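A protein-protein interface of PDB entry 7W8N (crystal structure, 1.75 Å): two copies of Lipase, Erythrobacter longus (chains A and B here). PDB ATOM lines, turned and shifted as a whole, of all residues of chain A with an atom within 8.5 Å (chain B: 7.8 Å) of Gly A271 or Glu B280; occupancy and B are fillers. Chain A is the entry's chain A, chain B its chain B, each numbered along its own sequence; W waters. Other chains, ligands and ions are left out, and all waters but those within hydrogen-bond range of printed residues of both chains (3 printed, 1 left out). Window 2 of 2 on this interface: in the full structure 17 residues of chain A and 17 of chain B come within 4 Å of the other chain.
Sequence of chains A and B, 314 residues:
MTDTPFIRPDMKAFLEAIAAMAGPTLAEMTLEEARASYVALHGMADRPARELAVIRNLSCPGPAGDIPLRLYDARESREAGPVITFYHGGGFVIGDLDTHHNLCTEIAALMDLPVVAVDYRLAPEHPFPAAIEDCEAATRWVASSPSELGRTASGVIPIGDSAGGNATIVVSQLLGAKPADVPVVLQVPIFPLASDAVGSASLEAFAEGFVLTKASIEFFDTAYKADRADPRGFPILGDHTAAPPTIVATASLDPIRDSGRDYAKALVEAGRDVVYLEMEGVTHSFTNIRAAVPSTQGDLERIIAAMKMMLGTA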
ATOM      1  N   HIS A 240     -24.204 -17.797  -7.858  1.00  0.00           N
ATOM      2  CA  HIS A 240     -23.053 -18.350  -8.581  1.00  0.00           C
ATOM      3  C   HIS A 240     -23.407 -18.940  -9.944  1.00  0.00           C
ATOM      4  O   HIS A 240     -22.504 -19.391 -10.664  1.00  0.00           O
ATOM      5  CB  HIS A 240     -22.392 -19.425  -7.731  1.00  0.00           C
ATOM      6  CG  HIS A 240     -22.137 -18.993  -6.332  1.00  0.00           C
ATOM      7  ND1 HIS A 240     -21.391 -17.873  -6.038  1.00  0.00           N
ATOM      8  CD2 HIS A 240     -22.559 -19.495  -5.153  1.00  0.00           C
ATOM      9  CE1 HIS A 240     -21.342 -17.717  -4.730  1.00  0.00           C
ATOM     10  NE2 HIS A 240     -22.051 -18.682  -4.167  1.00  0.00           N
ATOM     11  N   THR A 241     -24.687 -18.912 -10.335  1.00  0.00           N
ATOM     12  CA  THR A 241     -25.130 -19.679 -11.497  1.00  0.00           C
ATOM     13  C   THR A 241     -24.577 -19.169 -12.823  1.00  0.00           C
ATOM     14  O   THR A 241     -24.594 -19.926 -13.809  1.00  0.00           O
ATOM     15  CB  THR A 241     -26.671 -19.694 -11.572  1.00  0.00           C
ATOM     16  OG1 THR A 241     -27.150 -18.366 -11.725  1.00  0.00           O
ATOM     17  CG2 THR A 241     -27.264 -20.287 -10.326  1.00  0.00           C
ATOM     18  N   ALA A 242     -24.112 -17.927 -12.897  1.00  0.00           N
ATOM     19  CA  ALA A 242     -23.467 -17.407 -14.097  1.00  0.00           C
ATOM     20  C   ALA A 242     -22.046 -16.900 -13.826  1.00  0.00           C
ATOM     21  O   ALA A 242     -21.524 -16.064 -14.569  1.00  0.00           O
ATOM     22  CB  ALA A 242     -24.319 -16.306 -14.730  1.00  0.00           C
ATOM     23  N   ALA A 243     -21.398 -17.417 -12.788  1.00  0.00           N
ATOM     24  CA  ALA A 243     -20.047 -16.967 -12.480  1.00  0.00           C
ATOM     25  C   ALA A 243     -19.134 -17.155 -13.689  1.00  0.00           C
ATOM     26  O   ALA A 243     -19.203 -18.185 -14.377  1.00  0.00           O
ATOM     27  CB  ALA A 243     -19.474 -17.733 -11.282  1.00  0.00           C
ATOM     28  N   ALA A 264     -14.784 -22.278  -4.131  1.00  0.00           N
ATOM     29  CA  ALA A 264     -14.602 -23.152  -5.289  1.00  0.00           C
ATOM     30  C   ALA A 264     -15.625 -24.286  -5.297  1.00  0.00           C
ATOM     31  O   ALA A 264     -16.140 -24.654  -6.364  1.00  0.00           O
ATOM     32  CB  ALA A 264     -13.175 -23.703  -5.333  1.00  0.00           C
ATOM     33  N   LYS A 265     -15.955 -24.827  -4.124  1.00  0.00           N
ATOM     34  CA  LYS A 265     -17.003 -25.839  -4.039  1.00  0.00           C
ATOM     35  C   LYS A 265     -18.334 -25.291  -4.525  1.00  0.00           C
ATOM     36  O   LYS A 265     -19.085 -25.983  -5.225  1.00  0.00           O
ATOM     37  CB  LYS A 265     -17.141 -26.356  -2.614  1.00  0.00           C
ATOM     38  CG  LYS A 265     -15.977 -27.236  -2.195  1.00  0.00           C
ATOM     39  CD  LYS A 265     -16.023 -27.630  -0.712  1.00  0.00           C
ATOM     40  CE  LYS A 265     -17.227 -28.462  -0.369  1.00  0.00           C
ATOM     41  NZ  LYS A 265     -17.333 -28.662   1.097  1.00  0.00           N
ATOM     42  N   ALA A 266     -18.654 -24.054  -4.159  1.00  0.00           N
ATOM     43  CA  ALA A 266     -19.924 -23.477  -4.598  1.00  0.00           C
ATOM     44  C   ALA A 266     -19.965 -23.279  -6.105  1.00  0.00           C
ATOM     45  O   ALA A 266     -21.033 -23.405  -6.724  1.00  0.00           O
ATOM     46  CB  ALA A 266     -20.173 -22.129  -3.908  1.00  0.00           C
ATOM     47  N   LEU A 267     -18.835 -22.943  -6.709  1.00  0.00           N
ATOM     48  CA  LEU A 267     -18.795 -22.819  -8.153  1.00  0.00           C
ATOM     49  C   LEU A 267     -19.010 -24.175  -8.824  1.00  0.00           C
ATOM     50  O   LEU A 267     -19.765 -24.267  -9.793  1.00  0.00           O
ATOM     51  CB  LEU A 267     -17.473 -22.197  -8.604  1.00  0.00           C
ATOM     52  CG  LEU A 267     -17.238 -20.721  -8.241  1.00  0.00           C
ATOM     53  CD1 LEU A 267     -15.923 -20.205  -8.764  1.00  0.00           C
ATOM     54  CD2 LEU A 267     -18.335 -19.850  -8.772  1.00  0.00           C
ATOM     55  N   VAL A 268     -18.364 -25.232  -8.331  1.00  0.00           N
ATOM     56  CA  VAL A 268     -18.603 -26.570  -8.886  1.00  0.00           C
ATOM     57  C   VAL A 268     -20.069 -26.956  -8.708  1.00  0.00           C
ATOM     58  O   VAL A 268     -20.713 -27.488  -9.622  1.00  0.00           O
ATOM     59  CB  VAL A 268     -17.683 -27.610  -8.235  1.00  0.00           C
ATOM     60  CG1 VAL A 268     -18.074 -29.030  -8.686  1.00  0.00           C
ATOM     61  CG2 VAL A 268     -16.190 -27.321  -8.517  1.00  0.00           C
ATOM     62  N   GLU A 269     -20.610 -26.698  -7.518  1.00  0.00           N
ATOM     63  CA  GLU A 269     -22.007 -27.007  -7.232  1.00  0.00           C
ATOM     64  C   GLU A 269     -22.947 -26.342  -8.226  1.00  0.00           C
ATOM     65  O   GLU A 269     -23.988 -26.913  -8.584  1.00  0.00           O
ATOM     66  CB  GLU A 269     -22.340 -26.569  -5.799  1.00  0.00           C
ATOM     67  CG  GLU A 269     -23.820 -26.719  -5.411  1.00  0.00           C
ATOM     68  CD  GLU A 269     -24.283 -28.162  -5.436  1.00  0.00           C
ATOM     69  OE1 GLU A 269     -23.463 -29.062  -5.187  1.00  0.00           O
ATOM     70  OE2 GLU A 269     -25.478 -28.396  -5.706  1.00  0.00           O
ATOM     71  N   ALA A 270     -22.606 -25.129  -8.680  1.00  0.00           N
ATOM     72  CA  ALA A 270     -23.386 -24.396  -9.658  1.00  0.00           C
ATOM     73  C   ALA A 270     -23.004 -24.726 -11.102  1.00  0.00           C
ATOM     74  O   ALA A 270     -23.505 -24.089 -12.030  1.00  0.00           O
ATOM     75  CB  ALA A 270     -23.246 -22.879  -9.413  1.00  0.00           C
ATOM     76  N   GLY A 271     -22.106 -25.688 -11.319  1.00  0.00           N
ATOM     77  CA  GLY A 271     -21.752 -26.066 -12.677  1.00  0.00           C
ATOM     78  C   GLY A 271     -20.814 -25.136 -13.408  1.00  0.00           C
ATOM     79  O   GLY A 271     -20.790 -25.145 -14.639  1.00  0.00           O
ATOM     80  N   ARG A 272     -20.009 -24.351 -12.696  1.00  0.00           N
ATOM     81  CA  ARG A 272     -19.155 -23.348 -13.313  1.00  0.00           C
ATOM     82  C   ARG A 272     -17.735 -23.879 -13.455  1.00  0.00           C
ATOM     83  O   ARG A 272     -17.292 -24.690 -12.653  1.00  0.00           O
ATOM     84  CB  ARG A 272     -19.140 -22.066 -12.464  1.00  0.00           C
ATOM     85  CG  ARG A 272     -20.516 -21.588 -12.028  1.00  0.00           C
ATOM     86  CD  ARG A 272     -21.470 -21.457 -13.207  1.00  0.00           C
ATOM     87  NE  ARG A 272     -21.028 -20.485 -14.189  1.00  0.00           N
ATOM     88  CZ  ARG A 272     -21.359 -20.504 -15.479  1.00  0.00           C
ATOM     89  NH1 ARG A 272     -22.124 -21.477 -15.978  1.00  0.00           N
ATOM     90  NH2 ARG A 272     -20.910 -19.555 -16.283  1.00  0.00           N
ATOM     91  N   ASP A 273     -17.017 -23.383 -14.464  1.00  0.00           N
ATOM     92  CA  ASP A 273     -15.655 -23.845 -14.713  1.00  0.00           C
ATOM     93  C   ASP A 273     -14.728 -23.189 -13.702  1.00  0.00           C
ATOM     94  O   ASP A 273     -14.712 -21.959 -13.587  1.00  0.00           O
ATOM     95  CB  ASP A 273     -15.187 -23.477 -16.111  1.00  0.00           C
ATOM     96  CG  ASP A 273     -15.960 -24.201 -17.220  1.00  0.00           C
ATOM     97  OD1 ASP A 273     -16.666 -25.194 -16.947  1.00  0.00           O
ATOM     98  OD2 ASP A 273     -15.840 -23.755 -18.370  1.00  0.00           O
ATOM     99  N   VAL A 274     -13.921 -23.992 -13.025  1.00  0.00           N
ATOM    100  CA  VAL A 274     -13.033 -23.461 -11.985  1.00  0.00           C
ATOM    101  C   VAL A 274     -11.768 -24.306 -11.878  1.00  0.00           C
ATOM    102  O   VAL A 274     -11.794 -25.543 -11.963  1.00  0.00           O
ATOM    103  CB  VAL A 274     -13.763 -23.344 -10.625  1.00  0.00           C
ATOM    104  CG1 VAL A 274     -14.325 -24.658 -10.207  1.00  0.00           C
ATOM    105  CG2 VAL A 274     -12.803 -22.788  -9.533  1.00  0.00           C
ATOM    106  N   PHE B   6     -30.303 -25.644 -22.003  1.00  0.00           N
ATOM    107  CA  PHE B   6     -29.591 -25.239 -23.208  1.00  0.00           C
ATOM    108  C   PHE B   6     -28.950 -26.455 -23.882  1.00  0.00           C
ATOM    109  O   PHE B   6     -28.291 -27.267 -23.222  1.00  0.00           O
ATOM    110  CB  PHE B   6     -28.520 -24.202 -22.881  1.00  0.00           C
ATOM    111  CG  PHE B   6     -27.587 -23.942 -24.021  1.00  0.00           C
ATOM    112  CD1 PHE B   6     -28.017 -23.235 -25.131  1.00  0.00           C
ATOM    113  CD2 PHE B   6     -26.281 -24.429 -23.999  1.00  0.00           C
ATOM    114  CE1 PHE B   6     -27.165 -23.006 -26.191  1.00  0.00           C
ATOM    115  CE2 PHE B   6     -25.432 -24.203 -25.057  1.00  0.00           C
ATOM    116  CZ  PHE B   6     -25.870 -23.496 -26.153  1.00  0.00           C
ATOM    117  N   ILE B   7     -29.131 -26.555 -25.199  1.00  0.00           N
ATOM    118  CA  ILE B   7     -28.529 -27.593 -26.034  1.00  0.00           C
ATOM    119  C   ILE B   7     -27.960 -26.906 -27.260  1.00  0.00           C
ATOM    120  O   ILE B   7     -28.652 -26.104 -27.901  1.00  0.00           O
ATOM    121  CB  ILE B   7     -29.540 -28.672 -26.467  1.00  0.00           C
ATOM    122  CG1 ILE B   7     -30.362 -29.171 -25.276  1.00  0.00           C
ATOM    123  CG2 ILE B   7     -28.810 -29.815 -27.194  1.00  0.00           C
ATOM    124  CD1 ILE B   7     -31.553 -30.028 -25.667  1.00  0.00           C
ATOM    125  N   ARG B   8     -26.717 -27.229 -27.601  1.00  0.00           N
ATOM    126  CA  ARG B   8     -26.118 -26.674 -28.795  1.00  0.00           C
ATOM    127  C   ARG B   8     -26.895 -27.143 -30.024  1.00  0.00           C
ATOM    128  O   ARG B   8     -27.463 -28.237 -30.022  1.00  0.00           O
ATOM    129  CB  ARG B   8     -24.664 -27.104 -28.937  1.00  0.00           C
ATOM    130  CG  ARG B   8     -23.740 -26.582 -27.848  1.00  0.00           C
ATOM    131  CD  ARG B   8     -22.288 -26.956 -28.141  1.00  0.00           C
ATOM    132  NE  ARG B   8     -21.488 -26.846 -26.927  1.00  0.00           N
ATOM    133  CZ  ARG B   8     -20.316 -27.454 -26.731  1.00  0.00           C
ATOM    134  NH1 ARG B   8     -19.753 -28.196 -27.688  1.00  0.00           N
ATOM    135  NH2 ARG B   8     -19.693 -27.310 -25.574  1.00  0.00           N
ATOM    136  N   MET B  11     -25.585 -30.479 -31.341  1.00  0.00           N
ATOM    137  CA  MET B  11     -25.949 -31.519 -30.380  1.00  0.00           C
ATOM    138  C   MET B  11     -27.425 -31.887 -30.482  1.00  0.00           C
ATOM    139  O   MET B  11     -27.793 -33.072 -30.437  1.00  0.00           O
ATOM    140  CB  MET B  11     -25.640 -31.035 -28.956  1.00  0.00           C
ATOM    141  CG  MET B  11     -25.856 -32.069 -27.882  1.00  0.00           C
ATOM    142  SD  MET B  11     -24.438 -33.186 -27.772  1.00  0.00           S
ATOM    143  CE  MET B  11     -25.262 -34.766 -28.025  1.00  0.00           C
ATOM    144  N   THR B 250     -17.171 -32.795 -17.063  1.00  0.00           N
ATOM    145  CA  THR B 250     -18.536 -33.269 -17.096  1.00  0.00           C
ATOM    146  C   THR B 250     -19.258 -32.625 -18.273  1.00  0.00           C
ATOM    147  O   THR B 250     -18.712 -31.784 -19.002  1.00  0.00           O
ATOM    148  CB  THR B 250     -19.263 -32.929 -15.800  1.00  0.00           C
ATOM    149  OG1 THR B 250     -19.262 -31.502 -15.676  1.00  0.00           O
ATOM    150  CG2 THR B 250     -18.588 -33.610 -14.618  1.00  0.00           C
ATOM    151  N   ALA B 251     -20.517 -33.011 -18.452  1.00  0.00           N
ATOM    152  CA  ALA B 251     -21.382 -32.395 -19.445  1.00  0.00           C
ATOM    153  C   ALA B 251     -22.665 -31.905 -18.771  1.00  0.00           C
ATOM    154  O   ALA B 251     -23.208 -32.579 -17.893  1.00  0.00           O
ATOM    155  CB  ALA B 251     -21.711 -33.376 -20.556  1.00  0.00           C
ATOM    156  N   SER B 252     -23.140 -30.744 -19.203  1.00  0.00           N
ATOM    157  CA  SER B 252     -24.251 -30.088 -18.521  1.00  0.00           C
ATOM    158  C   SER B 252     -25.571 -30.836 -18.661  1.00  0.00           C
ATOM    159  O   SER B 252     -26.462 -30.638 -17.830  1.00  0.00           O
ATOM    160  CB  SER B 252     -24.432 -28.663 -19.032  1.00  0.00           C
ATOM    161  OG  SER B 252     -24.779 -28.588 -20.419  1.00  0.00           O
ATOM    162  N   LEU B 253     -25.734 -31.646 -19.710  1.00  0.00           N
ATOM    163  CA  LEU B 253     -26.943 -32.436 -19.935  1.00  0.00           C
ATOM    164  C   LEU B 253     -26.787 -33.905 -19.514  1.00  0.00           C
ATOM    165  O   LEU B 253     -27.589 -34.749 -19.920  1.00  0.00           O
ATOM    166  CB  LEU B 253     -27.330 -32.363 -21.416  1.00  0.00           C
ATOM    167  CG  LEU B 253     -27.461 -30.956 -21.982  1.00  0.00           C
ATOM    168  CD1 LEU B 253     -27.535 -30.991 -23.508  1.00  0.00           C
ATOM    169  CD2 LEU B 253     -28.692 -30.306 -21.380  1.00  0.00           C
ATOM    170  N   ARG B 257     -24.038 -36.047 -14.380  1.00  0.00           N
ATOM    171  CA  ARG B 257     -23.299 -34.804 -14.159  1.00  0.00           C
ATOM    172  C   ARG B 257     -23.039 -34.550 -12.679  1.00  0.00           C
ATOM    173  O   ARG B 257     -21.925 -34.172 -12.292  1.00  0.00           O
ATOM    174  CB  ARG B 257     -24.087 -33.644 -14.745  1.00  0.00           C
ATOM    175  CG  ARG B 257     -23.503 -32.243 -14.536  1.00  0.00           C
ATOM    176  CD  ARG B 257     -24.586 -31.230 -14.832  1.00  0.00           C
ATOM    177  NE  ARG B 257     -25.548 -31.223 -13.746  1.00  0.00           N
ATOM    178  CZ  ARG B 257     -26.677 -30.524 -13.762  1.00  0.00           C
ATOM    179  NH1 ARG B 257     -26.988 -29.813 -14.820  1.00  0.00           N
ATOM    180  NH2 ARG B 257     -27.486 -30.547 -12.710  1.00  0.00           N
ATOM    181  N   ASP B 258     -24.083 -34.663 -11.843  1.00  0.00           N
ATOM    182  CA  ASP B 258     -23.950 -34.320 -10.429  1.00  0.00           C
ATOM    183  C   ASP B 258     -22.963 -35.228  -9.707  1.00  0.00           C
ATOM    184  O   ASP B 258     -22.386 -34.820  -8.700  1.00  0.00           O
ATOM    185  CB  ASP B 258     -25.330 -34.358  -9.733  1.00  0.00           C
ATOM    186  CG  ASP B 258     -26.271 -33.245 -10.187  1.00  0.00           C
ATOM    187  OD1 ASP B 258     -25.873 -32.379 -10.998  1.00  0.00           O
ATOM    188  OD2 ASP B 258     -27.448 -33.236  -9.713  1.00  0.00           O
ATOM    189  N   ARG B 261     -19.721 -33.407 -10.373  1.00  0.00           N
ATOM    190  CA  ARG B 261     -19.701 -32.268  -9.457  1.00  0.00           C
ATOM    191  C   ARG B 261     -19.337 -32.705  -8.046  1.00  0.00           C
ATOM    192  O   ARG B 261     -18.488 -32.088  -7.378  1.00  0.00           O
ATOM    193  CB  ARG B 261     -21.071 -31.566  -9.458  1.00  0.00           C
ATOM    194  CG  ARG B 261     -21.365 -30.767 -10.703  1.00  0.00           C
ATOM    195  CD  ARG B 261     -22.769 -30.123 -10.614  1.00  0.00           C
ATOM    196  NE  ARG B 261     -23.131 -29.376 -11.810  1.00  0.00           N
ATOM    197  CZ  ARG B 261     -24.285 -28.727 -11.952  1.00  0.00           C
ATOM    198  NH1 ARG B 261     -25.181 -28.750 -10.977  1.00  0.00           N
ATOM    199  NH2 ARG B 261     -24.547 -28.072 -13.068  1.00  0.00           N
ATOM    200  N   TYR B 276     -12.115 -28.201 -12.752  1.00  0.00           N
ATOM    201  CA  TYR B 276     -13.486 -28.645 -13.004  1.00  0.00           C
ATOM    202  C   TYR B 276     -13.996 -27.963 -14.278  1.00  0.00           C
ATOM    203  O   TYR B 276     -14.102 -26.726 -14.349  1.00  0.00           O
ATOM    204  CB  TYR B 276     -14.413 -28.382 -11.795  1.00  0.00           C
ATOM    205  CG  TYR B 276     -15.788 -28.874 -12.091  1.00  0.00           C
ATOM    206  CD1 TYR B 276     -16.048 -30.238 -12.126  1.00  0.00           C
ATOM    207  CD2 TYR B 276     -16.811 -27.995 -12.431  1.00  0.00           C
ATOM    208  CE1 TYR B 276     -17.279 -30.721 -12.472  1.00  0.00           C
ATOM    209  CE2 TYR B 276     -18.063 -28.478 -12.794  1.00  0.00           C
ATOM    210  CZ  TYR B 276     -18.285 -29.851 -12.799  1.00  0.00           C
ATOM    211  OH  TYR B 276     -19.509 -30.374 -13.192  1.00  0.00           O
ATOM    212  N   LEU B 277     -14.286 -28.761 -15.308  1.00  0.00           N
ATOM    213  CA  LEU B 277     -14.802 -28.237 -16.567  1.00  0.00           C
ATOM    214  C   LEU B 277     -16.138 -28.900 -16.851  1.00  0.00           C
ATOM    215  O   LEU B 277     -16.212 -30.130 -16.964  1.00  0.00           O
ATOM    216  CB  LEU B 277     -13.838 -28.465 -17.737  1.00  0.00           C
ATOM    217  CG  LEU B 277     -12.428 -27.868 -17.633  1.00  0.00           C
ATOM    218  CD1 LEU B 277     -11.599 -28.332 -18.846  1.00  0.00           C
ATOM    219  CD2 LEU B 277     -12.420 -26.360 -17.519  1.00  0.00           C
ATOM    220  N   GLU B 278     -17.186 -28.085 -16.979  1.00  0.00           N
ATOM    221  CA  GLU B 278     -18.533 -28.583 -17.246  1.00  0.00           C
ATOM    222  C   GLU B 278     -18.918 -28.056 -18.623  1.00  0.00           C
ATOM    223  O   GLU B 278     -19.139 -26.855 -18.805  1.00  0.00           O
ATOM    224  CB  GLU B 278     -19.526 -28.171 -16.152  1.00  0.00           C
ATOM    225  CG  GLU B 278     -20.944 -28.704 -16.401  1.00  0.00           C
ATOM    226  CD  GLU B 278     -21.868 -28.609 -15.199  1.00  0.00           C
ATOM    227  OE1 GLU B 278     -21.467 -28.985 -14.090  1.00  0.00           O
ATOM    228  OE2 GLU B 278     -23.031 -28.196 -15.392  1.00  0.00           O
ATOM    229  N   MET B 279     -18.907 -28.950 -19.614  1.00  0.00           N
ATOM    230  CA  MET B 279     -19.114 -28.555 -20.994  1.00  0.00           C
ATOM    231  C   MET B 279     -20.586 -28.209 -21.214  1.00  0.00           C
ATOM    232  O   MET B 279     -21.466 -28.993 -20.863  1.00  0.00           O
ATOM    233  CB  MET B 279     -18.692 -29.690 -21.931  1.00  0.00           C
ATOM    234  CG  MET B 279     -17.300 -30.195 -21.668  1.00  0.00           C
ATOM    235  SD  MET B 279     -16.057 -28.899 -21.790  1.00  0.00           S
ATOM    236  CE  MET B 279     -14.571 -29.835 -21.372  1.00  0.00           C
ATOM    237  N   GLU B 280     -20.838 -27.046 -21.798  1.00  0.00           N
ATOM    238  CA  GLU B 280     -22.182 -26.465 -21.837  1.00  0.00           C
ATOM    239  C   GLU B 280     -22.922 -26.884 -23.103  1.00  0.00           C
ATOM    240  O   GLU B 280     -22.437 -26.653 -24.216  1.00  0.00           O
ATOM    241  CB  GLU B 280     -22.116 -24.944 -21.770  1.00  0.00           C
ATOM    242  CG  GLU B 280     -21.686 -24.428 -20.427  1.00  0.00           C
ATOM    243  CD  GLU B 280     -22.652 -24.830 -19.328  1.00  0.00           C
ATOM    244  OE1 GLU B 280     -23.862 -25.004 -19.624  1.00  0.00           O
ATOM    245  OE2 GLU B 280     -22.203 -24.968 -18.165  1.00  0.00           O
ATOM    246  N   GLY B 281     -24.101 -27.467 -22.923  1.00  0.00           N
ATOM    247  CA  GLY B 281     -25.004 -27.744 -24.019  1.00  0.00           C
ATOM    248  C   GLY B 281     -24.685 -29.019 -24.760  1.00  0.00           C
ATOM    249  O   GLY B 281     -25.106 -29.175 -25.915  1.00  0.00           O
ATOM    250  N   VAL B 282     -23.931 -29.929 -24.133  1.00  0.00           N
ATOM    251  CA  VAL B 282     -23.598 -31.217 -24.721  1.00  0.00           C
ATOM    252  C   VAL B 282     -23.875 -32.304 -23.696  1.00  0.00           C
ATOM    253  O   VAL B 282     -24.064 -32.054 -22.509  1.00  0.00           O
ATOM    254  CB  VAL B 282     -22.139 -31.290 -25.219  1.00  0.00           C
ATOM    255  CG1 VAL B 282     -21.918 -30.326 -26.376  1.00  0.00           C
ATOM    256  CG2 VAL B 282     -21.154 -31.014 -24.059  1.00  0.00           C
ATOM    257  N   THR B 283     -23.972 -33.514 -24.171  1.00  0.00           N
ATOM    258  CA  THR B 283     -24.369 -34.627 -23.323  1.00  0.00           C
ATOM    259  C   THR B 283     -23.142 -35.397 -22.877  1.00  0.00           C
ATOM    260  O   THR B 283     -22.105 -35.288 -23.412  1.00  0.00           O
ATOM    261  CB  THR B 283     -25.326 -35.493 -24.164  1.00  0.00           C
ATOM    262  OG1 THR B 283     -24.513 -35.990 -25.215  1.00  0.00           O
ATOM    263  CG2 THR B 283     -26.546 -34.721 -24.572  1.00  0.00           C
ATOM    264  N   PHE B 286     -19.622 -37.092 -25.084  1.00  0.00           N
ATOM    265  CA  PHE B 286     -19.188 -36.114 -26.076  1.00  0.00           C
ATOM    266  C   PHE B 286     -17.796 -36.410 -26.641  1.00  0.00           C
ATOM    267  O   PHE B 286     -17.501 -35.966 -27.752  1.00  0.00           O
ATOM    268  CB  PHE B 286     -19.267 -34.674 -25.541  1.00  0.00           C
ATOM    269  CG  PHE B 286     -18.292 -34.325 -24.423  1.00  0.00           C
ATOM    270  CD1 PHE B 286     -16.974 -33.984 -24.716  1.00  0.00           C
ATOM    271  CD2 PHE B 286     -18.725 -34.240 -23.105  1.00  0.00           C
ATOM    272  CE1 PHE B 286     -16.068 -33.641 -23.682  1.00  0.00           C
ATOM    273  CE2 PHE B 286     -17.839 -33.877 -22.066  1.00  0.00           C
ATOM    274  CZ  PHE B 286     -16.511 -33.576 -22.368  1.00  0.00           C
ATOM    275  N   SER B 295     -18.803 -29.610 -32.704  1.00  0.00           N
ATOM    276  CA  SER B 295     -18.370 -28.733 -31.619  1.00  0.00           C
ATOM    277  C   SER B 295     -17.749 -29.508 -30.464  1.00  0.00           C
ATOM    278  O   SER B 295     -17.033 -28.906 -29.654  1.00  0.00           O
ATOM    279  CB  SER B 295     -19.551 -27.876 -31.126  1.00  0.00           C
ATOM    280  OG  SER B 295     -20.560 -28.663 -30.490  1.00  0.00           O
ATOM    281  N   ASP B 299     -14.509 -29.345 -27.186  1.00  0.00           N
ATOM    282  CA  ASP B 299     -14.565 -29.759 -25.785  1.00  0.00           C
ATOM    283  C   ASP B 299     -13.392 -30.676 -25.445  1.00  0.00           C
ATOM    284  O   ASP B 299     -12.738 -30.505 -24.411  1.00  0.00           O
ATOM    285  CB  ASP B 299     -15.883 -30.471 -25.466  1.00  0.00           C
ATOM    286  CG  ASP B 299     -17.115 -29.610 -25.748  1.00  0.00           C
ATOM    287  OD1 ASP B 299     -17.114 -28.429 -25.345  1.00  0.00           O
ATOM    288  OD2 ASP B 299     -18.083 -30.120 -26.383  1.00  0.00           O
ATOM    289  N   ARG B 302     -10.274 -28.600 -25.060  1.00  0.00           N
ATOM    290  CA  ARG B 302     -10.143 -27.902 -23.775  1.00  0.00           C
ATOM    291  C   ARG B 302      -9.585 -28.831 -22.705  1.00  0.00           C
ATOM    292  O   ARG B 302      -8.770 -28.409 -21.872  1.00  0.00           O
ATOM    293  CB  ARG B 302     -11.493 -27.332 -23.316  1.00  0.00           C
ATOM    294  CG  ARG B 302     -12.039 -26.288 -24.249  1.00  0.00           C
ATOM    295  CD  ARG B 302     -13.370 -25.746 -23.697  1.00  0.00           C
ATOM    296  NE  ARG B 302     -13.206 -25.159 -22.372  1.00  0.00           N
ATOM    297  CZ  ARG B 302     -14.188 -24.990 -21.497  1.00  0.00           C
ATOM    298  NH1 ARG B 302     -15.430 -25.375 -21.788  1.00  0.00           N
ATOM    299  NH2 ARG B 302     -13.926 -24.421 -20.321  1.00  0.00           N
HETATM  300  O   HOH W   1     -17.687 -24.858 -19.951  1.00  0.00           O
HETATM  301  O   HOH W   2     -15.250 -21.478 -19.041  1.00  0.00           O
HETATM  302  O   HOH W   3     -25.219 -29.996  -8.213  1.00  0.00           O
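Of the 15 printed residues of chain A, 6 touch a printed residue of chain B.
Printed residues of chain A that touch a printed residue of chain B: Val A268, Glu A269, Gly A271, Arg A272, Asp A273 and Val A274.
Hydrophobic or aromatic side chains of chain A within 4 Å of the printed part of chain B: Val A268.
Of the 23 printed residues of chain B, 6 touch a printed residue of chain A.
Hydrophobic or aromatic side chains of chain B that line the printed part of chain A: Tyr B276.
Among the printed residues, 12 pairs touch across the chains.
The side-chain carboxylate (OD1) of Asp A273 is in hydrogen-bond range of the backbone NH (N) of Glu B278 (2.9 Å).
The backbone carbonyl oxygen (O) of Val A274 is in hydrogen-bond range of the backbone NH (N) of Tyr B276.
The side-chain carboxylate of Asp A273 is in salt-bridge range of the guanidinium group of Arg B302 (2.8 Å).
NH1 of Arg B261 sits at hydrogen-bond distance from O of Glu A269 (3.2 Å).
Among the printed residues, pairs that only touch across the chains: Gly A271 with Glu B278, Asp A273 with Tyr B276, Arg A272 with Tyr B276, Val A268 with Arg B261, Gly A271 with Arg B261, Asp A273 with Leu B277, Gly A271 with Glu B280 and Val A268 with Tyr B276.
Of the printed residues of chain B, Val A268 touches Arg B261 and Tyr B276.
No residue of chain B comes within 4 Å of Ala A270.
Gly A271 touches just these residues of chain B: Arg B261, Glu B278 and Glu B280.
Arg B8 touches none of the printed residues of chain A.
Thr B250 touches none of the printed residues of chain A.
Of the printed residues of chain A, Leu B277 touches Asp A273 (3.6 Å).
Glu B280 touches one residue of chain A.
No residue of chain A comes within 4 Å of Gly B281.
Water W2 lies within hydrogen-bond range of OD2 of Asp A273 (2.4 Å) and NH2 of Arg B302 (3.5 Å).
Water W1 lies within hydrogen-bond range of the side-chain carboxylate of Asp A273 (2.7 Å), the backbone carbonyl oxygen of Glu B278 (2.7 Å) and the guanidinium group of Arg B302 (3.0 Å).
Water W3 lies within hydrogen-bond range of the side-chain carboxylate of Glu A269 and the guanidinium group of Arg B261.
The backbone carbonyl oxygen (O) of Glu B280 is in hydrogen-bond range of the guanidinium group (NE) of Arg B8.
The backbone NH of Thr B250 is in hydrogen-bond range of the backbone carbonyl oxygen of Leu B277 (2.8 Å).
OE1 of Glu B278 is in hydrogen-bond range of OH of Tyr B276 (2.6 Å).
The guanidinium group (NH2) of Arg B261 is in salt-bridge range of the side-chain carboxylate (OE2) of Glu B278, at 2.8 Å.
The backbone NH of Arg A272 lies within hydrogen-bond range of the backbone carbonyl oxygen of Leu A267.
The guanidinium group of Arg A272 sits at hydrogen-bond distance from the backbone carbonyl oxygen of Ala A243 (2.9 Å).
No position is printed for both chains.
Of the 12 pairs that touch across the chains among the printed residues, none has its exchanged pair printed and touching as well.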
